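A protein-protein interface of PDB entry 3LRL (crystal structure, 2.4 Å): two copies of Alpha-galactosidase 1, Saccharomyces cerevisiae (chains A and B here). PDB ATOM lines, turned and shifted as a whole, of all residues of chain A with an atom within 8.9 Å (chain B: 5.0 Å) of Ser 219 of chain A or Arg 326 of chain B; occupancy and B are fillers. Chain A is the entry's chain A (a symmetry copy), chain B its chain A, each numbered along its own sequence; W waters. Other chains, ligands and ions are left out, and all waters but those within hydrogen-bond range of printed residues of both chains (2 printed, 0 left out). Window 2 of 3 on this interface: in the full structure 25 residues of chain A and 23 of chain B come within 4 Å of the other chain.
Of the printed residues of chain B, Arg 216 of chain A touches Val 327.
Ser 219 of chain A touches just these residues of chain B: Pro 248 (3.3 Å), Thr 325 (3.7 Å) and Arg 326 (2.8 Å).
Of the printed residues of chain B, Arg 220 of chain A touches Thr 325.
Of the printed residues of chain B, Pro 222 of chain A touches Pro 248.
Of the printed residues of chain B, Tyr 232 of chain A touches Pro 248 (3.1 Å).
Pro 248 of chain B touches just these residues of chain A: Ser 219 (3.3 Å), Pro 222 (3.98 Å) and Tyr 232 (3.1 Å).
Printed residues of chain A within 4 Å of Arg 326 of chain B: Ser 219 (2.8 Å).
Printed residues of chain A within 4 Å of Val 327 of chain B: Arg 216 (3.3 Å).
Gln 344 of chain B touches none of the printed residues of chain A.
The nearest residue of chain A that does not touch Arg 326 of chain B is Asp 218 of chain A (5.3 Å).
Among the printed residues, merely in contact across the chains: Ser 219 of chain A with Pro 248 of chain B, Arg 220 of chain A with Thr 325 of chain B, Ser 219 of chain A with Thr 325 of chain B and Pro 222 of chain A with Pro 248 of chain B.
No position is printed for both chains.
Water W2 lies within hydrogen-bond range of the backbone carbonyl oxygen of Ala 247 of chain B (2.6 Å), the side-chain hydroxyl of Ser 219 of chain A (2.7 Å) and the backbone NH of Arg 326 of chain B (2.9 Å).
Water W1 lies within hydrogen-bond range of O of Arg 326 of chain B, O of Val 327 of chain B, NH1 of Arg 216 of chain A and N of Ser 219 of chain A.
SG of Cys 221 of chain A is disulfide-bonded to SG of Cys 237 of chain A (2.0 Å).
The guanidinium group (NH1) of Arg 216 of chain A is in salt-bridge range of the side-chain carboxylate (OD2) of Asp 218 of chain A, at 3.6 Å.
N of Val 327 of chain B is in hydrogen-bond range of O of Met 345 of chain B (2.7 Å).
The guanidinium group (NH1) of Arg 220 of chain A lies within hydrogen-bond range of a ring nitrogen (NE2) of His 236 of chain A.
O of Arg 220 of chain A is in hydrogen-bond range of N of Phe 235 of chain A, 2.9 Å away.
The side-chain carboxylate (OD1) of Asp 218 of chain A is in salt-bridge range of the guanidinium group (NE) of Arg 220 of chain A (2.9 Å).
Of the 12 printed residues of chain B, 4 touch a printed residue of chain A.
Printed residues of chain B that touch a printed residue of chain A: Pro 248, Thr 325, Arg 326 and Val 327.
Hydrophobic or aromatic side chains of chain B that line the printed part of chain A: Pro 248 and Val 327.
Among the printed residues, no Asp or Glu carboxylate lies within 4 Å of a Lys or Arg side-chain nitrogen of the other chain.
The guanidinium group of Arg 216 of chain A sits at hydrogen-bond distance from the backbone carbonyl oxygen of Val 327 of chain B, at 3.3 Å.
The backbone carbonyl oxygen (O) of Pro 248 of chain B sits at hydrogen-bond distance from the side-chain hydroxyl (OH) of Tyr 232 of chain A, at 3.1 Å.
O of Arg 326 of chain B lies within hydrogen-bond range of OG of Ser 219 of chain A, 2.8 Å away.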
ATOM      1  N   ARG A 216      -2.823  23.435  25.666  1.00  0.00           N
ATOM      2  CA  ARG A 216      -4.279  23.498  25.541  1.00  0.00           C
ATOM      3  C   ARG A 216      -5.041  22.358  26.249  1.00  0.00           C
ATOM      4  O   ARG A 216      -4.955  21.191  25.840  1.00  0.00           O
ATOM      5  CB  ARG A 216      -4.697  23.566  24.062  1.00  0.00           C
ATOM      6  CG  ARG A 216      -6.173  23.954  23.833  1.00  0.00           C
ATOM      7  CD  ARG A 216      -6.636  23.598  22.431  1.00  0.00           C
ATOM      8  NE  ARG A 216      -7.956  24.133  22.090  1.00  0.00           N
ATOM      9  CZ  ARG A 216      -9.134  23.592  22.439  1.00  0.00           C
ATOM     10  NH1 ARG A 216      -9.200  22.485  23.173  1.00  0.00           N
ATOM     11  NH2 ARG A 216     -10.269  24.176  22.069  1.00  0.00           N
ATOM     12  N   PRO A 217      -5.803  22.699  27.298  1.00  0.00           N
ATOM     13  CA  PRO A 217      -6.747  21.694  27.806  1.00  0.00           C
ATOM     14  C   PRO A 217      -7.780  21.280  26.737  1.00  0.00           C
ATOM     15  O   PRO A 217      -8.200  22.090  25.900  1.00  0.00           O
ATOM     16  CB  PRO A 217      -7.420  22.390  28.993  1.00  0.00           C
ATOM     17  CG  PRO A 217      -6.471  23.549  29.360  1.00  0.00           C
ATOM     18  CD  PRO A 217      -5.850  23.964  28.061  1.00  0.00           C
ATOM     19  N   ASP A 218      -8.165  20.014  26.765  1.00  0.00           N
ATOM     20  CA  ASP A 218      -9.059  19.465  25.770  1.00  0.00           C
ATOM     21  C   ASP A 218     -10.030  18.530  26.470  1.00  0.00           C
ATOM     22  O   ASP A 218      -9.651  17.821  27.409  1.00  0.00           O
ATOM     23  CB  ASP A 218      -8.262  18.736  24.681  1.00  0.00           C
ATOM     24  CG  ASP A 218      -9.079  18.473  23.430  1.00  0.00           C
ATOM     25  OD1 ASP A 218     -10.054  17.705  23.474  1.00  0.00           O
ATOM     26  OD2 ASP A 218      -8.719  18.998  22.369  1.00  0.00           O
ATOM     27  N   SER A 219     -11.287  18.560  26.034  1.00  0.00           N
ATOM     28  CA  SER A 219     -12.356  17.798  26.706  1.00  0.00           C
ATOM     29  C   SER A 219     -12.268  16.307  26.369  1.00  0.00           C
ATOM     30  O   SER A 219     -12.906  15.460  27.026  1.00  0.00           O
ATOM     31  CB  SER A 219     -13.722  18.347  26.326  1.00  0.00           C
ATOM     32  OG  SER A 219     -13.948  18.219  24.935  1.00  0.00           O
ATOM     33  N   ARG A 220     -11.482  16.001  25.339  1.00  0.00           N
ATOM     34  CA  ARG A 220     -11.198  14.614  24.930  1.00  0.00           C
ATOM     35  C   ARG A 220     -10.023  14.010  25.739  1.00  0.00           C
ATOM     36  O   ARG A 220      -9.699  12.829  25.616  1.00  0.00           O
ATOM     37  CB  ARG A 220     -10.931  14.552  23.420  1.00  0.00           C
ATOM     38  CG  ARG A 220     -12.107  15.052  22.576  1.00  0.00           C
ATOM     39  CD  ARG A 220     -11.722  15.317  21.134  1.00  0.00           C
ATOM     40  NE  ARG A 220     -10.881  16.504  20.985  1.00  0.00           N
ATOM     41  CZ  ARG A 220     -10.376  16.923  19.824  1.00  0.00           C
ATOM     42  NH1 ARG A 220     -10.627  16.245  18.704  1.00  0.00           N
ATOM     43  NH2 ARG A 220      -9.631  18.024  19.772  1.00  0.00           N
ATOM     44  N   CYS A 221      -9.405  14.848  26.560  1.00  0.00           N
ATOM     45  CA  CYS A 221      -8.356  14.464  27.492  1.00  0.00           C
ATOM     46  C   CYS A 221      -8.775  14.973  28.883  1.00  0.00           C
ATOM     47  O   CYS A 221      -8.252  15.963  29.351  1.00  0.00           O
ATOM     48  CB  CYS A 221      -7.027  15.080  27.027  1.00  0.00           C
ATOM     49  SG  CYS A 221      -5.578  14.648  27.975  1.00  0.00           S
ATOM     50  N   PRO A 222      -9.745  14.296  29.534  1.00  0.00           N
ATOM     51  CA  PRO A 222     -10.323  14.802  30.796  1.00  0.00           C
ATOM     52  C   PRO A 222      -9.361  14.863  31.983  1.00  0.00           C
ATOM     53  O   PRO A 222      -9.627  15.597  32.940  1.00  0.00           O
ATOM     54  CB  PRO A 222     -11.438  13.796  31.109  1.00  0.00           C
ATOM     55  CG  PRO A 222     -11.038  12.530  30.368  1.00  0.00           C
ATOM     56  CD  PRO A 222     -10.346  13.000  29.129  1.00  0.00           C
ATOM     57  N   CYS A 223      -8.272  14.093  31.959  1.00  0.00           N
ATOM     58  CA  CYS A 223      -7.352  14.119  33.075  1.00  0.00           C
ATOM     59  C   CYS A 223      -6.378  15.245  32.913  1.00  0.00           C
ATOM     60  O   CYS A 223      -5.762  15.369  31.854  1.00  0.00           O
ATOM     61  CB  CYS A 223      -6.607  12.802  33.197  1.00  0.00           C
ATOM     62  SG  CYS A 223      -7.690  11.439  33.636  1.00  0.00           S
ATOM     63  N   TYR A 232      -9.553   7.724  32.276  1.00  0.00           N
ATOM     64  CA  TYR A 232      -9.977   7.988  30.909  1.00  0.00           C
ATOM     65  C   TYR A 232      -8.845   8.747  30.233  1.00  0.00           C
ATOM     66  O   TYR A 232      -8.901   9.975  30.153  1.00  0.00           O
ATOM     67  CB  TYR A 232     -11.260   8.839  30.882  1.00  0.00           C
ATOM     68  CG  TYR A 232     -12.099   8.712  29.603  1.00  0.00           C
ATOM     69  CD1 TYR A 232     -13.416   9.214  29.557  1.00  0.00           C
ATOM     70  CD2 TYR A 232     -11.586   8.094  28.445  1.00  0.00           C
ATOM     71  CE1 TYR A 232     -14.201   9.095  28.408  1.00  0.00           C
ATOM     72  CE2 TYR A 232     -12.356   7.971  27.286  1.00  0.00           C
ATOM     73  CZ  TYR A 232     -13.668   8.477  27.277  1.00  0.00           C
ATOM     74  OH  TYR A 232     -14.446   8.356  26.144  1.00  0.00           O
ATOM     75  N   ALA A 233      -7.827   8.013  29.772  1.00  0.00           N
ATOM     76  CA  ALA A 233      -6.628   8.600  29.149  1.00  0.00           C
ATOM     77  C   ALA A 233      -6.966   9.570  28.009  1.00  0.00           C
ATOM     78  O   ALA A 233      -6.370  10.648  27.903  1.00  0.00           O
ATOM     79  CB  ALA A 233      -5.685   7.503  28.640  1.00  0.00           C
ATOM     80  N   GLY A 234      -7.903   9.154  27.161  1.00  0.00           N
ATOM     81  CA  GLY A 234      -8.364   9.966  26.036  1.00  0.00           C
ATOM     82  C   GLY A 234      -7.291  10.271  25.027  1.00  0.00           C
ATOM     83  O   GLY A 234      -6.375   9.468  24.801  1.00  0.00           O
ATOM     84  N   PHE A 235      -7.412  11.436  24.400  1.00  0.00           N
ATOM     85  CA  PHE A 235      -6.396  11.916  23.445  1.00  0.00           C
ATOM     86  C   PHE A 235      -6.534  13.421  23.228  1.00  0.00           C
ATOM     87  O   PHE A 235      -7.307  14.073  23.923  1.00  0.00           O
ATOM     88  CB  PHE A 235      -6.373  11.105  22.123  1.00  0.00           C
ATOM     89  CG  PHE A 235      -7.612  11.250  21.235  1.00  0.00           C
ATOM     90  CD1 PHE A 235      -7.502  11.025  19.855  1.00  0.00           C
ATOM     91  CD2 PHE A 235      -8.869  11.552  21.759  1.00  0.00           C
ATOM     92  CE1 PHE A 235      -8.613  11.113  19.011  1.00  0.00           C
ATOM     93  CE2 PHE A 235     -10.006  11.659  20.924  1.00  0.00           C
ATOM     94  CZ  PHE A 235      -9.890  11.438  19.559  1.00  0.00           C
ATOM     95  N   HIS A 236      -5.769  13.965  22.288  1.00  0.00           N
ATOM     96  CA  HIS A 236      -5.650  15.416  22.124  1.00  0.00           C
ATOM     97  C   HIS A 236      -5.177  16.088  23.408  1.00  0.00           C
ATOM     98  O   HIS A 236      -5.646  17.160  23.754  1.00  0.00           O
ATOM     99  CB  HIS A 236      -6.951  16.030  21.589  1.00  0.00           C
ATOM    100  CG  HIS A 236      -7.308  15.551  20.211  1.00  0.00           C
ATOM    101  ND1 HIS A 236      -6.784  16.114  19.065  1.00  0.00           N
ATOM    102  CD2 HIS A 236      -8.112  14.544  19.796  1.00  0.00           C
ATOM    103  CE1 HIS A 236      -7.254  15.479  18.005  1.00  0.00           C
ATOM    104  NE2 HIS A 236      -8.065  14.525  18.422  1.00  0.00           N
ATOM    105  N   CYS A 237      -4.241  15.447  24.103  1.00  0.00           N
ATOM    106  CA  CYS A 237      -3.671  15.971  25.342  1.00  0.00           C
ATOM    107  C   CYS A 237      -2.549  16.876  24.934  1.00  0.00           C
ATOM    108  O   CYS A 237      -1.861  16.583  23.969  1.00  0.00           O
ATOM    109  CB  CYS A 237      -3.104  14.841  26.216  1.00  0.00           C
ATOM    110  SG  CYS A 237      -4.315  13.603  26.747  1.00  0.00           S
ATOM    111  N   ASN B 244     -22.660  17.083  30.785  1.00  0.00           N
ATOM    112  CA  ASN B 244     -21.302  17.349  31.223  1.00  0.00           C
ATOM    113  C   ASN B 244     -20.488  16.057  31.398  1.00  0.00           C
ATOM    114  O   ASN B 244     -19.315  16.008  31.020  1.00  0.00           O
ATOM    115  CB  ASN B 244     -21.336  18.194  32.493  1.00  0.00           C
ATOM    116  CG  ASN B 244     -21.606  19.662  32.211  1.00  0.00           C
ATOM    117  OD1 ASN B 244     -21.385  20.138  31.111  1.00  0.00           O
ATOM    118  ND2 ASN B 244     -22.089  20.381  33.210  1.00  0.00           N
ATOM    119  N   ALA B 247     -19.492  14.464  27.967  1.00  0.00           N
ATOM    120  CA  ALA B 247     -18.576  15.253  27.128  1.00  0.00           C
ATOM    121  C   ALA B 247     -17.254  14.577  26.740  1.00  0.00           C
ATOM    122  O   ALA B 247     -16.852  14.691  25.594  1.00  0.00           O
ATOM    123  CB  ALA B 247     -18.327  16.672  27.729  1.00  0.00           C
ATOM    124  N   PRO B 248     -16.540  13.929  27.699  1.00  0.00           N
ATOM    125  CA  PRO B 248     -15.292  13.244  27.265  1.00  0.00           C
ATOM    126  C   PRO B 248     -15.537  11.961  26.494  1.00  0.00           C
ATOM    127  O   PRO B 248     -14.622  11.481  25.801  1.00  0.00           O
ATOM    128  CB  PRO B 248     -14.571  12.936  28.586  1.00  0.00           C
ATOM    129  CG  PRO B 248     -15.670  12.840  29.608  1.00  0.00           C
ATOM    130  CD  PRO B 248     -16.734  13.835  29.169  1.00  0.00           C
ATOM    131  N   ALA B 324     -20.132  15.175  18.503  1.00  0.00           N
ATOM    132  CA  ALA B 324     -19.408  16.447  18.519  1.00  0.00           C
ATOM    133  C   ALA B 324     -18.540  16.555  19.773  1.00  0.00           C
ATOM    134  O   ALA B 324     -18.784  15.857  20.765  1.00  0.00           O
ATOM    135  CB  ALA B 324     -20.378  17.647  18.443  1.00  0.00           C
ATOM    136  N   THR B 325     -17.564  17.467  19.713  1.00  0.00           N
ATOM    137  CA  THR B 325     -16.612  17.717  20.762  1.00  0.00           C
ATOM    138  C   THR B 325     -16.929  19.027  21.482  1.00  0.00           C
ATOM    139  O   THR B 325     -17.305  20.021  20.845  1.00  0.00           O
ATOM    140  CB  THR B 325     -15.193  17.828  20.146  1.00  0.00           C
ATOM    141  OG1 THR B 325     -14.875  16.607  19.471  1.00  0.00           O
ATOM    142  CG2 THR B 325     -14.119  18.137  21.207  1.00  0.00           C
ATOM    143  N   ARG B 326     -16.763  19.044  22.804  1.00  0.00           N
ATOM    144  CA  ARG B 326     -16.887  20.306  23.532  1.00  0.00           C
ATOM    145  C   ARG B 326     -15.595  21.051  23.258  1.00  0.00           C
ATOM    146  O   ARG B 326     -14.493  20.546  23.560  1.00  0.00           O
ATOM    147  CB  ARG B 326     -17.087  20.091  25.043  1.00  0.00           C
ATOM    148  CG  ARG B 326     -17.751  21.281  25.735  1.00  0.00           C
ATOM    149  CD  ARG B 326     -17.220  21.498  27.138  1.00  0.00           C
ATOM    150  NE  ARG B 326     -17.963  20.731  28.120  1.00  0.00           N
ATOM    151  CZ  ARG B 326     -17.433  20.108  29.172  1.00  0.00           C
ATOM    152  NH1 ARG B 326     -16.137  20.121  29.413  1.00  0.00           N
ATOM    153  NH2 ARG B 326     -18.221  19.458  29.988  1.00  0.00           N
ATOM    154  N   VAL B 327     -15.714  22.225  22.645  1.00  0.00           N
ATOM    155  CA  VAL B 327     -14.538  22.996  22.318  1.00  0.00           C
ATOM    156  C   VAL B 327     -14.130  23.774  23.562  1.00  0.00           C
ATOM    157  O   VAL B 327     -12.964  23.745  23.955  1.00  0.00           O
ATOM    158  CB  VAL B 327     -14.722  23.899  21.073  1.00  0.00           C
ATOM    159  CG1 VAL B 327     -13.417  24.619  20.743  1.00  0.00           C
ATOM    160  CG2 VAL B 327     -15.172  23.072  19.881  1.00  0.00           C
ATOM    161  N   TRP B 328     -15.092  24.433  24.198  1.00  0.00           N
ATOM    162  CA  TRP B 328     -14.803  25.156  25.427  1.00  0.00           C
ATOM    163  C   TRP B 328     -15.972  25.214  26.392  1.00  0.00           C
ATOM    164  O   TRP B 328     -17.123  24.949  26.008  1.00  0.00           O
ATOM    165  CB  TRP B 328     -14.218  26.559  25.174  1.00  0.00           C
ATOM    166  CG  TRP B 328     -14.949  27.483  24.213  1.00  0.00           C
ATOM    167  CD1 TRP B 328     -14.529  27.841  22.963  1.00  0.00           C
ATOM    168  CD2 TRP B 328     -16.159  28.240  24.458  1.00  0.00           C
ATOM    169  NE1 TRP B 328     -15.403  28.744  22.408  1.00  0.00           N
ATOM    170  CE2 TRP B 328     -16.410  29.009  23.298  1.00  0.00           C
ATOM    171  CE3 TRP B 328     -17.056  28.327  25.531  1.00  0.00           C
ATOM    172  CZ2 TRP B 328     -17.526  29.856  23.175  1.00  0.00           C
ATOM    173  CZ3 TRP B 328     -18.178  29.162  25.410  1.00  0.00           C
ATOM    174  CH2 TRP B 328     -18.399  29.912  24.239  1.00  0.00           C
ATOM    175  N   ARG B 329     -15.649  25.537  27.648  1.00  0.00           N
ATOM    176  CA  ARG B 329     -16.639  25.638  28.706  1.00  0.00           C
ATOM    177  C   ARG B 329     -16.169  26.680  29.706  1.00  0.00           C
ATOM    178  O   ARG B 329     -15.027  26.603  30.182  1.00  0.00           O
ATOM    179  CB  ARG B 329     -16.853  24.273  29.380  1.00  0.00           C
ATOM    180  CG  ARG B 329     -17.973  24.238  30.409  1.00  0.00           C
ATOM    181  CD  ARG B 329     -17.464  24.528  31.820  1.00  0.00           C
ATOM    182  NE  ARG B 329     -16.621  23.465  32.391  1.00  0.00           N
ATOM    183  CZ  ARG B 329     -17.075  22.311  32.879  1.00  0.00           C
ATOM    184  NH1 ARG B 329     -18.361  22.019  32.838  1.00  0.00           N
ATOM    185  NH2 ARG B 329     -16.232  21.436  33.397  1.00  0.00           N
ATOM    186  N   GLN B 344     -21.002  27.020  26.919  1.00  0.00           N
ATOM    187  CA  GLN B 344     -20.239  25.981  26.213  1.00  0.00           C
ATOM    188  C   GLN B 344     -20.330  26.180  24.708  1.00  0.00           C
ATOM    189  O   GLN B 344     -21.311  26.740  24.196  1.00  0.00           O
ATOM    190  CB  GLN B 344     -20.740  24.576  26.585  1.00  0.00           C
ATOM    191  CG  GLN B 344     -20.544  24.215  28.080  1.00  0.00           C
ATOM    192  CD  GLN B 344     -21.167  22.874  28.507  1.00  0.00           C
ATOM    193  OE1 GLN B 344     -21.763  22.146  27.698  1.00  0.00           O
ATOM    194  NE2 GLN B 344     -21.028  22.552  29.787  1.00  0.00           N
ATOM    195  N   MET B 345     -19.281  25.746  24.020  1.00  0.00           N
ATOM    196  CA  MET B 345     -19.261  25.670  22.566  1.00  0.00           C
ATOM    197  C   MET B 345     -18.904  24.252  22.209  1.00  0.00           C
ATOM    198  O   MET B 345     -17.913  23.728  22.706  1.00  0.00           O
ATOM    199  CB  MET B 345     -18.189  26.575  21.975  1.00  0.00           C
ATOM    200  CG  MET B 345     -18.480  27.011  20.561  1.00  0.00           C
ATOM    201  SD  MET B 345     -17.044  27.165  19.493  1.00  0.00           S
ATOM    202  CE  MET B 345     -17.373  25.741  18.486  1.00  0.00           C
ATOM    203  N   TRP B 346     -19.713  23.647  21.347  1.00  0.00           N
ATOM    204  CA  TRP B 346     -19.464  22.320  20.828  1.00  0.00           C
ATOM    205  C   TRP B 346     -19.381  22.417  19.323  1.00  0.00           C
ATOM    206  O   TRP B 346     -20.034  23.246  18.727  1.00  0.00           O
ATOM    207  CB  TRP B 346     -20.613  21.358  21.168  1.00  0.00           C
ATOM    208  CG  TRP B 346     -20.805  21.007  22.637  1.00  0.00           C
ATOM    209  CD1 TRP B 346     -21.224  21.849  23.629  1.00  0.00           C
ATOM    210  CD2 TRP B 346     -20.645  19.717  23.250  1.00  0.00           C
ATOM    211  NE1 TRP B 346     -21.318  21.170  24.819  1.00  0.00           N
ATOM    212  CE2 TRP B 346     -20.961  19.862  24.618  1.00  0.00           C
ATOM    213  CE3 TRP B 346     -20.259  18.456  22.779  1.00  0.00           C
ATOM    214  CZ2 TRP B 346     -20.908  18.788  25.526  1.00  0.00           C
ATOM    215  CZ3 TRP B 346     -20.203  17.380  23.694  1.00  0.00           C
ATOM    216  CH2 TRP B 346     -20.519  17.562  25.045  1.00  0.00           C
HETATM  217  O   HOH W   1     -11.924  20.879  23.863  1.00  0.00           O
HETATM  218  O   HOH W   2     -15.864  16.531  24.034  1.00  0.00           O
